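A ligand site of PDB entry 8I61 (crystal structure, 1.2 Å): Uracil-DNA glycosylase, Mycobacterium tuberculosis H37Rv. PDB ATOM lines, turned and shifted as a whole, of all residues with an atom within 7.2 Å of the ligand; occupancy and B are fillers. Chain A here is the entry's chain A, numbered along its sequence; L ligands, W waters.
The backbone NH (N) of Gln 78 lies within hydrogen-bond range of an oxygen (O1) of the ligand (2.8 Å). The backbone NH of Phe 92 lies within hydrogen-bond range of an oxygen (O2) of the ligand (2.8 Å). A nitrogen (N2) of the ligand is in hydrogen-bond range of the side-chain amide oxygen of Asn 138 (2.9 Å). N2 of the ligand sits at hydrogen-bond distance from O of Asp 79. NE2 of His 202 lies within hydrogen-bond range of O1 of the ligand, at 2.8 Å.
The side-chain amide nitrogen of Gln 78 sits at hydrogen-bond distance from the side-chain carboxylate of Asp 79, at 2.9 Å. A ring nitrogen (ND1) of His 202 is in hydrogen-bond range of the backbone NH (N) of Ser 204 (2.9 Å). The backbone carbonyl oxygen (O) of Leu 136 sits at hydrogen-bond distance from the backbone NH (N) of Ser 91. The backbone carbonyl oxygen (O) of Gln 78 is in hydrogen-bond range of the backbone NH (N) of Arg 139. N of Val 140 lies within hydrogen-bond range of O of Gln 78. The backbone carbonyl oxygen of Gly 77 sits at hydrogen-bond distance from the backbone NH of Arg 139, 2.9 Å away. N of Gly 77 lies within hydrogen-bond range of O of Leu 137, at 3.0 Å. OG of Ser 91 sits at hydrogen-bond distance from O of Leu 137 (3.0 Å).
C of Gly 77 touches O1 of the ligand (3.6 Å). C of Pro 80 touches C3 of the ligand, at 3.8 Å. CD1 of Tyr 81 touches O3 of the ligand (3.2 Å). Ser 91 touches the ligand. Along chain A the residues within 4 Å of the ligand span positions 77 to 202. The nearest printed residue that does not touch the ligand is Pro 82 (4.1 Å).
Water W3 bridges OG of Ser 104 and O3 of the ligand. Water W4 bridges O2 of the ligand (2.7 Å) and N of Tyr 81 (3.0 Å). Water W2 lies within hydrogen-bond range of N1 of the ligand and NE2 of His 202.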
ATOM      1  N   VAL A  76     -31.976   6.360  15.554  1.00  0.00           N
ATOM      2  CA  VAL A  76     -31.409   5.298  16.389  1.00  0.00           C
ATOM      3  C   VAL A  76     -30.384   4.552  15.568  1.00  0.00           C
ATOM      4  O   VAL A  76     -30.705   3.989  14.514  1.00  0.00           O
ATOM      5  CB  VAL A  76     -32.452   4.364  16.943  1.00  0.00           C
ATOM      6  CG1 VAL A  76     -31.791   3.423  17.957  1.00  0.00           C
ATOM      7  CG2 VAL A  76     -33.645   5.098  17.576  1.00  0.00           C
ATOM      8  N   GLY A  77     -29.158   4.558  16.071  1.00  0.00           N
ATOM      9  CA  GLY A  77     -28.132   3.658  15.586  1.00  0.00           C
ATOM     10  C   GLY A  77     -27.820   2.509  16.531  1.00  0.00           C
ATOM     11  O   GLY A  77     -28.724   2.135  17.379  1.00  0.00           O
ATOM     12  N   GLN A  78     -26.656   1.941  16.392  1.00  0.00           N
ATOM     13  CA  GLN A  78     -26.242   0.699  17.020  1.00  0.00           C
ATOM     14  C   GLN A  78     -25.575   0.961  18.379  1.00  0.00           C
ATOM     15  O   GLN A  78     -26.089   0.549  19.460  1.00  0.00           O
ATOM     16  CB  GLN A  78     -25.307  -0.132  16.128  1.00  0.00           C
ATOM     17  CG  GLN A  78     -24.779  -1.371  16.826  1.00  0.00           C
ATOM     18  CD  GLN A  78     -23.882  -2.141  15.896  1.00  0.00           C
ATOM     19  OE1 GLN A  78     -24.378  -2.879  15.060  1.00  0.00           O
ATOM     20  NE2 GLN A  78     -22.595  -1.928  16.048  1.00  0.00           N
ATOM     21  N   ASP A  79     -24.454   1.634  18.355  1.00  0.00           N
ATOM     22  CA  ASP A  79     -23.633   1.894  19.560  1.00  0.00           C
ATOM     23  C   ASP A  79     -22.630   2.974  19.177  1.00  0.00           C
ATOM     24  O   ASP A  79     -22.526   3.357  18.012  1.00  0.00           O
ATOM     25  CB  ASP A  79     -22.954   0.596  20.072  1.00  0.00           C
ATOM     26  CG  ASP A  79     -21.905  -0.046  19.209  1.00  0.00           C
ATOM     27  OD1 ASP A  79     -21.926   0.139  17.998  1.00  0.00           O
ATOM     28  OD2 ASP A  79     -21.080  -0.742  19.804  1.00  0.00           O
ATOM     29  N   PRO A  80     -21.891   3.548  20.136  1.00  0.00           N
ATOM     30  CA  PRO A  80     -21.064   4.708  19.808  1.00  0.00           C
ATOM     31  C   PRO A  80     -19.829   4.410  18.964  1.00  0.00           C
ATOM     32  O   PRO A  80     -19.398   3.242  18.812  1.00  0.00           O
ATOM     33  CB  PRO A  80     -20.585   5.195  21.163  1.00  0.00           C
ATOM     34  CG  PRO A  80     -21.623   4.690  22.177  1.00  0.00           C
ATOM     35  CD  PRO A  80     -22.031   3.336  21.591  1.00  0.00           C
ATOM     36  N   TYR A  81     -19.287   5.458  18.356  1.00  0.00           N
ATOM     37  CA  TYR A  81     -18.087   5.263  17.550  1.00  0.00           C
ATOM     38  C   TYR A  81     -17.025   4.547  18.359  1.00  0.00           C
ATOM     39  O   TYR A  81     -16.799   4.878  19.495  1.00  0.00           O
ATOM     40  CB  TYR A  81     -17.518   6.587  17.063  1.00  0.00           C
ATOM     41  CG  TYR A  81     -18.304   7.330  16.004  1.00  0.00           C
ATOM     42  CD1 TYR A  81     -18.414   6.781  14.750  1.00  0.00           C
ATOM     43  CD2 TYR A  81     -18.913   8.544  16.267  1.00  0.00           C
ATOM     44  CE1 TYR A  81     -19.157   7.394  13.780  1.00  0.00           C
ATOM     45  CE2 TYR A  81     -19.638   9.200  15.268  1.00  0.00           C
ATOM     46  CZ  TYR A  81     -19.753   8.610  14.016  1.00  0.00           C
ATOM     47  OH  TYR A  81     -20.440   9.204  12.978  1.00  0.00           O
ATOM     48  N   PRO A  82     -16.275   3.638  17.732  1.00  0.00           N
ATOM     49  CA  PRO A  82     -15.291   2.833  18.475  1.00  0.00           C
ATOM     50  C   PRO A  82     -13.916   3.529  18.636  1.00  0.00           C
ATOM     51  O   PRO A  82     -13.081   3.018  19.349  1.00  0.00           O
ATOM     52  CB  PRO A  82     -15.195   1.574  17.617  1.00  0.00           C
ATOM     53  CG  PRO A  82     -15.442   2.067  16.212  1.00  0.00           C
ATOM     54  CD  PRO A  82     -16.563   3.067  16.413  1.00  0.00           C
ATOM     55  N   ALA A  87     -16.789   9.509  19.593  1.00  0.00           N
ATOM     56  CA  ALA A  87     -18.123   9.480  20.227  1.00  0.00           C
ATOM     57  C   ALA A  87     -18.258  10.644  21.221  1.00  0.00           C
ATOM     58  O   ALA A  87     -17.358  10.866  22.053  1.00  0.00           O
ATOM     59  CB  ALA A  87     -18.332   8.179  20.928  1.00  0.00           C
ATOM     60  N   VAL A  88     -19.410  11.303  21.138  1.00  0.00           N
ATOM     61  CA  VAL A  88     -19.704  12.435  22.038  1.00  0.00           C
ATOM     62  C   VAL A  88     -21.016  12.235  22.802  1.00  0.00           C
ATOM     63  O   VAL A  88     -21.475  13.187  23.467  1.00  0.00           O
ATOM     64  CB  VAL A  88     -19.702  13.766  21.263  1.00  0.00           C
ATOM     65  CG1 VAL A  88     -18.363  14.061  20.629  1.00  0.00           C
ATOM     66  CG2 VAL A  88     -20.838  13.882  20.263  1.00  0.00           C
ATOM     67  N   GLY A  89     -21.658  11.080  22.722  1.00  0.00           N
ATOM     68  CA  GLY A  89     -22.915  10.821  23.430  1.00  0.00           C
ATOM     69  C   GLY A  89     -24.150  11.227  22.650  1.00  0.00           C
ATOM     70  O   GLY A  89     -25.296  11.091  23.147  1.00  0.00           O
ATOM     71  N   LEU A  90     -23.994  11.735  21.431  1.00  0.00           N
ATOM     72  CA  LEU A  90     -25.080  11.965  20.465  1.00  0.00           C
ATOM     73  C   LEU A  90     -24.778  11.050  19.302  1.00  0.00           C
ATOM     74  O   LEU A  90     -23.715  11.172  18.732  1.00  0.00           O
ATOM     75  CB  LEU A  90     -25.144  13.432  20.025  1.00  0.00           C
ATOM     76  CG  LEU A  90     -25.470  14.425  21.144  1.00  0.00           C
ATOM     77  CD1 LEU A  90     -25.353  15.852  20.647  1.00  0.00           C
ATOM     78  CD2 LEU A  90     -26.849  14.132  21.763  1.00  0.00           C
ATOM     79  N   SER A  91     -25.712  10.191  18.937  1.00  0.00           N
ATOM     80  CA  SER A  91     -25.409   9.207  17.893  1.00  0.00           C
ATOM     81  C   SER A  91     -24.934   9.907  16.635  1.00  0.00           C
ATOM     82  O   SER A  91     -25.505  10.948  16.161  1.00  0.00           O
ATOM     83  CB  SER A  91     -26.558   8.292  17.654  1.00  0.00           C
ATOM     84  OG  SER A  91     -27.671   8.949  17.129  1.00  0.00           O
ATOM     85  N   PHE A  92     -23.884   9.346  16.044  1.00  0.00           N
ATOM     86  CA  PHE A  92     -23.234   9.735  14.761  1.00  0.00           C
ATOM     87  C   PHE A  92     -22.526  11.078  14.814  1.00  0.00           C
ATOM     88  O   PHE A  92     -21.740  11.363  13.886  1.00  0.00           O
ATOM     89  CB  PHE A  92     -24.193   9.646  13.586  1.00  0.00           C
ATOM     90  CG  PHE A  92     -24.773   8.260  13.466  1.00  0.00           C
ATOM     91  CD1 PHE A  92     -24.016   7.268  12.879  1.00  0.00           C
ATOM     92  CD2 PHE A  92     -26.043   7.963  13.885  1.00  0.00           C
ATOM     93  CE1 PHE A  92     -24.543   5.996  12.716  1.00  0.00           C
ATOM     94  CE2 PHE A  92     -26.558   6.676  13.793  1.00  0.00           C
ATOM     95  CZ  PHE A  92     -25.787   5.703  13.221  1.00  0.00           C
ATOM     96  N   SER A  93     -22.740  11.897  15.818  1.00  0.00           N
ATOM     97  CA  SER A  93     -22.112  13.204  15.883  1.00  0.00           C
ATOM     98  C   SER A  93     -20.640  13.145  16.236  1.00  0.00           C
ATOM     99  O   SER A  93     -20.208  12.227  17.000  1.00  0.00           O
ATOM    100  CB  SER A  93     -22.843  14.016  16.915  1.00  0.00           C
ATOM    101  OG  SER A  93     -22.586  15.431  16.750  1.00  0.00           O
ATOM    102  N   PRO A 102     -15.717  10.250  10.510  1.00  0.00           N
ATOM    103  CA  PRO A 102     -15.926   8.799  10.470  1.00  0.00           C
ATOM    104  C   PRO A 102     -16.668   8.443   9.164  1.00  0.00           C
ATOM    105  O   PRO A 102     -17.495   9.193   8.646  1.00  0.00           O
ATOM    106  CB  PRO A 102     -16.808   8.526  11.701  1.00  0.00           C
ATOM    107  CG  PRO A 102     -16.510   9.634  12.616  1.00  0.00           C
ATOM    108  CD  PRO A 102     -16.298  10.832  11.726  1.00  0.00           C
ATOM    109  N   SER A 104     -19.079   6.309   8.526  1.00  0.00           N
ATOM    110  CA  SER A 104     -20.570   6.272   8.650  1.00  0.00           C
ATOM    111  C   SER A 104     -21.140   7.677   8.472  1.00  0.00           C
ATOM    112  O   SER A 104     -22.158   7.876   7.826  1.00  0.00           O
ATOM    113  CB  SER A 104     -21.071   5.716   9.953  1.00  0.00           C
ATOM    114  OG  SER A 104     -20.869   4.319  10.028  1.00  0.00           O
ATOM    115  N   LEU A 136     -30.785  11.917  19.158  1.00  0.00           N
ATOM    116  CA  LEU A 136     -29.690  11.183  18.513  1.00  0.00           C
ATOM    117  C   LEU A 136     -29.265  10.010  19.421  1.00  0.00           C
ATOM    118  O   LEU A 136     -28.340  10.132  20.219  1.00  0.00           O
ATOM    119  CB  LEU A 136     -28.545  12.172  18.220  1.00  0.00           C
ATOM    120  CG  LEU A 136     -28.906  13.321  17.296  1.00  0.00           C
ATOM    121  CD1 LEU A 136     -27.777  14.287  17.174  1.00  0.00           C
ATOM    122  CD2 LEU A 136     -29.280  12.760  15.983  1.00  0.00           C
ATOM    123  N   LEU A 137     -30.033   8.948  19.310  1.00  0.00           N
ATOM    124  CA  LEU A 137     -29.912   7.784  20.207  1.00  0.00           C
ATOM    125  C   LEU A 137     -29.111   6.669  19.545  1.00  0.00           C
ATOM    126  O   LEU A 137     -29.078   6.536  18.331  1.00  0.00           O
ATOM    127  CB  LEU A 137     -31.322   7.315  20.576  1.00  0.00           C
ATOM    128  CG  LEU A 137     -31.419   6.343  21.755  1.00  0.00           C
ATOM    129  CD1 LEU A 137     -30.933   6.997  23.021  1.00  0.00           C
ATOM    130  CD2 LEU A 137     -32.865   5.899  21.910  1.00  0.00           C
ATOM    131  N   ASN A 138     -28.465   5.840  20.337  1.00  0.00           N
ATOM    132  CA  ASN A 138     -27.961   4.528  19.956  1.00  0.00           C
ATOM    133  C   ASN A 138     -28.689   3.470  20.786  1.00  0.00           C
ATOM    134  O   ASN A 138     -29.079   3.763  21.939  1.00  0.00           O
ATOM    135  CB  ASN A 138     -26.451   4.434  20.161  1.00  0.00           C
ATOM    136  CG  ASN A 138     -25.668   5.101  19.052  1.00  0.00           C
ATOM    137  OD1 ASN A 138     -25.991   4.907  17.882  1.00  0.00           O
ATOM    138  ND2 ASN A 138     -24.648   5.883  19.389  1.00  0.00           N
ATOM    139  N   ARG A 139     -28.859   2.294  20.229  1.00  0.00           N
ATOM    140  CA  ARG A 139     -29.514   1.211  20.985  1.00  0.00           C
ATOM    141  C   ARG A 139     -28.735   0.840  22.235  1.00  0.00           C
ATOM    142  O   ARG A 139     -29.322   0.542  23.338  1.00  0.00           O
ATOM    143  CB  ARG A 139     -29.646  -0.017  20.084  1.00  0.00           C
ATOM    144  CG  ARG A 139     -30.521  -1.100  20.684  1.00  0.00           C
ATOM    145  CD  ARG A 139     -31.997  -0.751  20.554  1.00  0.00           C
ATOM    146  NE  ARG A 139     -32.819  -1.873  20.858  1.00  0.00           N
ATOM    147  CZ  ARG A 139     -33.260  -2.208  22.060  1.00  0.00           C
ATOM    148  NH1 ARG A 139     -33.141  -1.405  23.094  1.00  0.00           N
ATOM    149  NH2 ARG A 139     -33.941  -3.322  22.173  1.00  0.00           N
ATOM    150  N   VAL A 140     -27.411   0.941  22.152  1.00  0.00           N
ATOM    151  CA  VAL A 140     -26.465   0.647  23.232  1.00  0.00           C
ATOM    152  C   VAL A 140     -25.605   1.912  23.414  1.00  0.00           C
ATOM    153  O   VAL A 140     -25.200   2.491  22.404  1.00  0.00           O
ATOM    154  CB  VAL A 140     -25.663  -0.619  22.928  1.00  0.00           C
ATOM    155  CG1 VAL A 140     -24.425  -0.791  23.785  1.00  0.00           C
ATOM    156  CG2 VAL A 140     -26.609  -1.818  22.992  1.00  0.00           C
ATOM    157  N   PRO A 148     -16.545  -2.448  17.963  1.00  0.00           N
ATOM    158  CA  PRO A 148     -17.986  -2.259  17.773  1.00  0.00           C
ATOM    159  C   PRO A 148     -18.811  -3.424  18.296  1.00  0.00           C
ATOM    160  O   PRO A 148     -18.404  -4.600  18.176  1.00  0.00           O
ATOM    161  CB  PRO A 148     -18.168  -2.146  16.261  1.00  0.00           C
ATOM    162  CG  PRO A 148     -16.811  -1.664  15.785  1.00  0.00           C
ATOM    163  CD  PRO A 148     -15.791  -2.294  16.711  1.00  0.00           C
ATOM    164  N   TRP A 179     -31.698   2.961  12.015  1.00  0.00           N
ATOM    165  CA  TRP A 179     -30.577   2.619  11.112  1.00  0.00           C
ATOM    166  C   TRP A 179     -29.866   1.383  11.611  1.00  0.00           C
ATOM    167  O   TRP A 179     -29.201   1.398  12.663  1.00  0.00           O
ATOM    168  CB  TRP A 179     -29.585   3.778  11.028  1.00  0.00           C
ATOM    169  CG  TRP A 179     -30.061   4.922  10.165  1.00  0.00           C
ATOM    170  CD1 TRP A 179     -30.997   4.893   9.175  1.00  0.00           C
ATOM    171  CD2 TRP A 179     -29.618   6.281  10.212  1.00  0.00           C
ATOM    172  NE1 TRP A 179     -31.178   6.136   8.599  1.00  0.00           N
ATOM    173  CE2 TRP A 179     -30.305   7.008   9.208  1.00  0.00           C
ATOM    174  CE3 TRP A 179     -28.609   6.946  10.902  1.00  0.00           C
ATOM    175  CZ2 TRP A 179     -30.108   8.362   8.991  1.00  0.00           C
ATOM    176  CZ3 TRP A 179     -28.410   8.272  10.717  1.00  0.00           C
ATOM    177  CH2 TRP A 179     -29.144   8.970   9.766  1.00  0.00           C
ATOM    178  N   HIS A 202     -27.902   0.180   7.979  1.00  0.00           N
ATOM    179  CA  HIS A 202     -26.988   1.084   8.680  1.00  0.00           C
ATOM    180  C   HIS A 202     -26.103   1.792   7.658  1.00  0.00           C
ATOM    181  O   HIS A 202     -25.649   1.220   6.650  1.00  0.00           O
ATOM    182  CB  HIS A 202     -26.207   0.261   9.697  1.00  0.00           C
ATOM    183  CG  HIS A 202     -25.446   1.098  10.671  1.00  0.00           C
ATOM    184  ND1 HIS A 202     -24.244   1.673  10.393  1.00  0.00           N
ATOM    185  CD2 HIS A 202     -25.765   1.398  11.978  1.00  0.00           C
ATOM    186  CE1 HIS A 202     -23.860   2.304  11.474  1.00  0.00           C
ATOM    187  NE2 HIS A 202     -24.762   2.157  12.486  1.00  0.00           N
ATOM    188  N   PRO A 203     -25.726   3.071   7.952  1.00  0.00           N
ATOM    189  CA  PRO A 203     -24.854   3.822   7.045  1.00  0.00           C
ATOM    190  C   PRO A 203     -23.362   3.451   7.070  1.00  0.00           C
ATOM    191  O   PRO A 203     -22.605   3.958   6.266  1.00  0.00           O
ATOM    192  CB  PRO A 203     -25.031   5.267   7.515  1.00  0.00           C
ATOM    193  CG  PRO A 203     -25.446   5.148   8.948  1.00  0.00           C
ATOM    194  CD  PRO A 203     -26.346   3.938   8.969  1.00  0.00           C
ATOM    195  N   SER A 204     -22.958   2.522   7.912  1.00  0.00           N
ATOM    196  CA  SER A 204     -21.566   1.997   7.882  1.00  0.00           C
ATOM    197  C   SER A 204     -21.245   1.503   6.495  1.00  0.00           C
ATOM    198  O   SER A 204     -22.132   0.934   5.807  1.00  0.00           O
ATOM    199  CB  SER A 204     -21.495   0.874   8.867  1.00  0.00           C
ATOM    200  OG  SER A 204     -20.568  -0.097   8.543  1.00  0.00           O
HETATM  201  N1  LIG L   1     -22.390   3.707  14.761  1.00  0.00           N
HETATM  202  C1  LIG L   1     -23.634   3.920  15.292  1.00  0.00           C
HETATM  203  O1  LIG L   1     -24.570   3.155  15.049  1.00  0.00           O
HETATM  204  N2  LIG L   1     -23.791   5.063  16.013  1.00  0.00           N
HETATM  205  C2  LIG L   1     -22.805   5.945  16.366  1.00  0.00           C
HETATM  206  O2  LIG L   1     -23.045   6.858  17.142  1.00  0.00           O
HETATM  207  C3  LIG L   1     -21.532   5.682  15.789  1.00  0.00           C
HETATM  208  C4  LIG L   1     -21.274   4.421  15.089  1.00  0.00           C
HETATM  209  O3  LIG L   1     -20.140   4.087  14.714  1.00  0.00           O
HETATM  210  O   HOH W   1     -19.377   1.441  14.907  1.00  0.00           O
HETATM  211  O   HOH W   2     -21.944   1.054  13.914  1.00  0.00           O
HETATM  212  O   HOH W   3     -19.568   3.537  12.140  1.00  0.00           O
HETATM  213  O   HOH W   4     -21.057   7.815  18.751  1.00  0.00           O
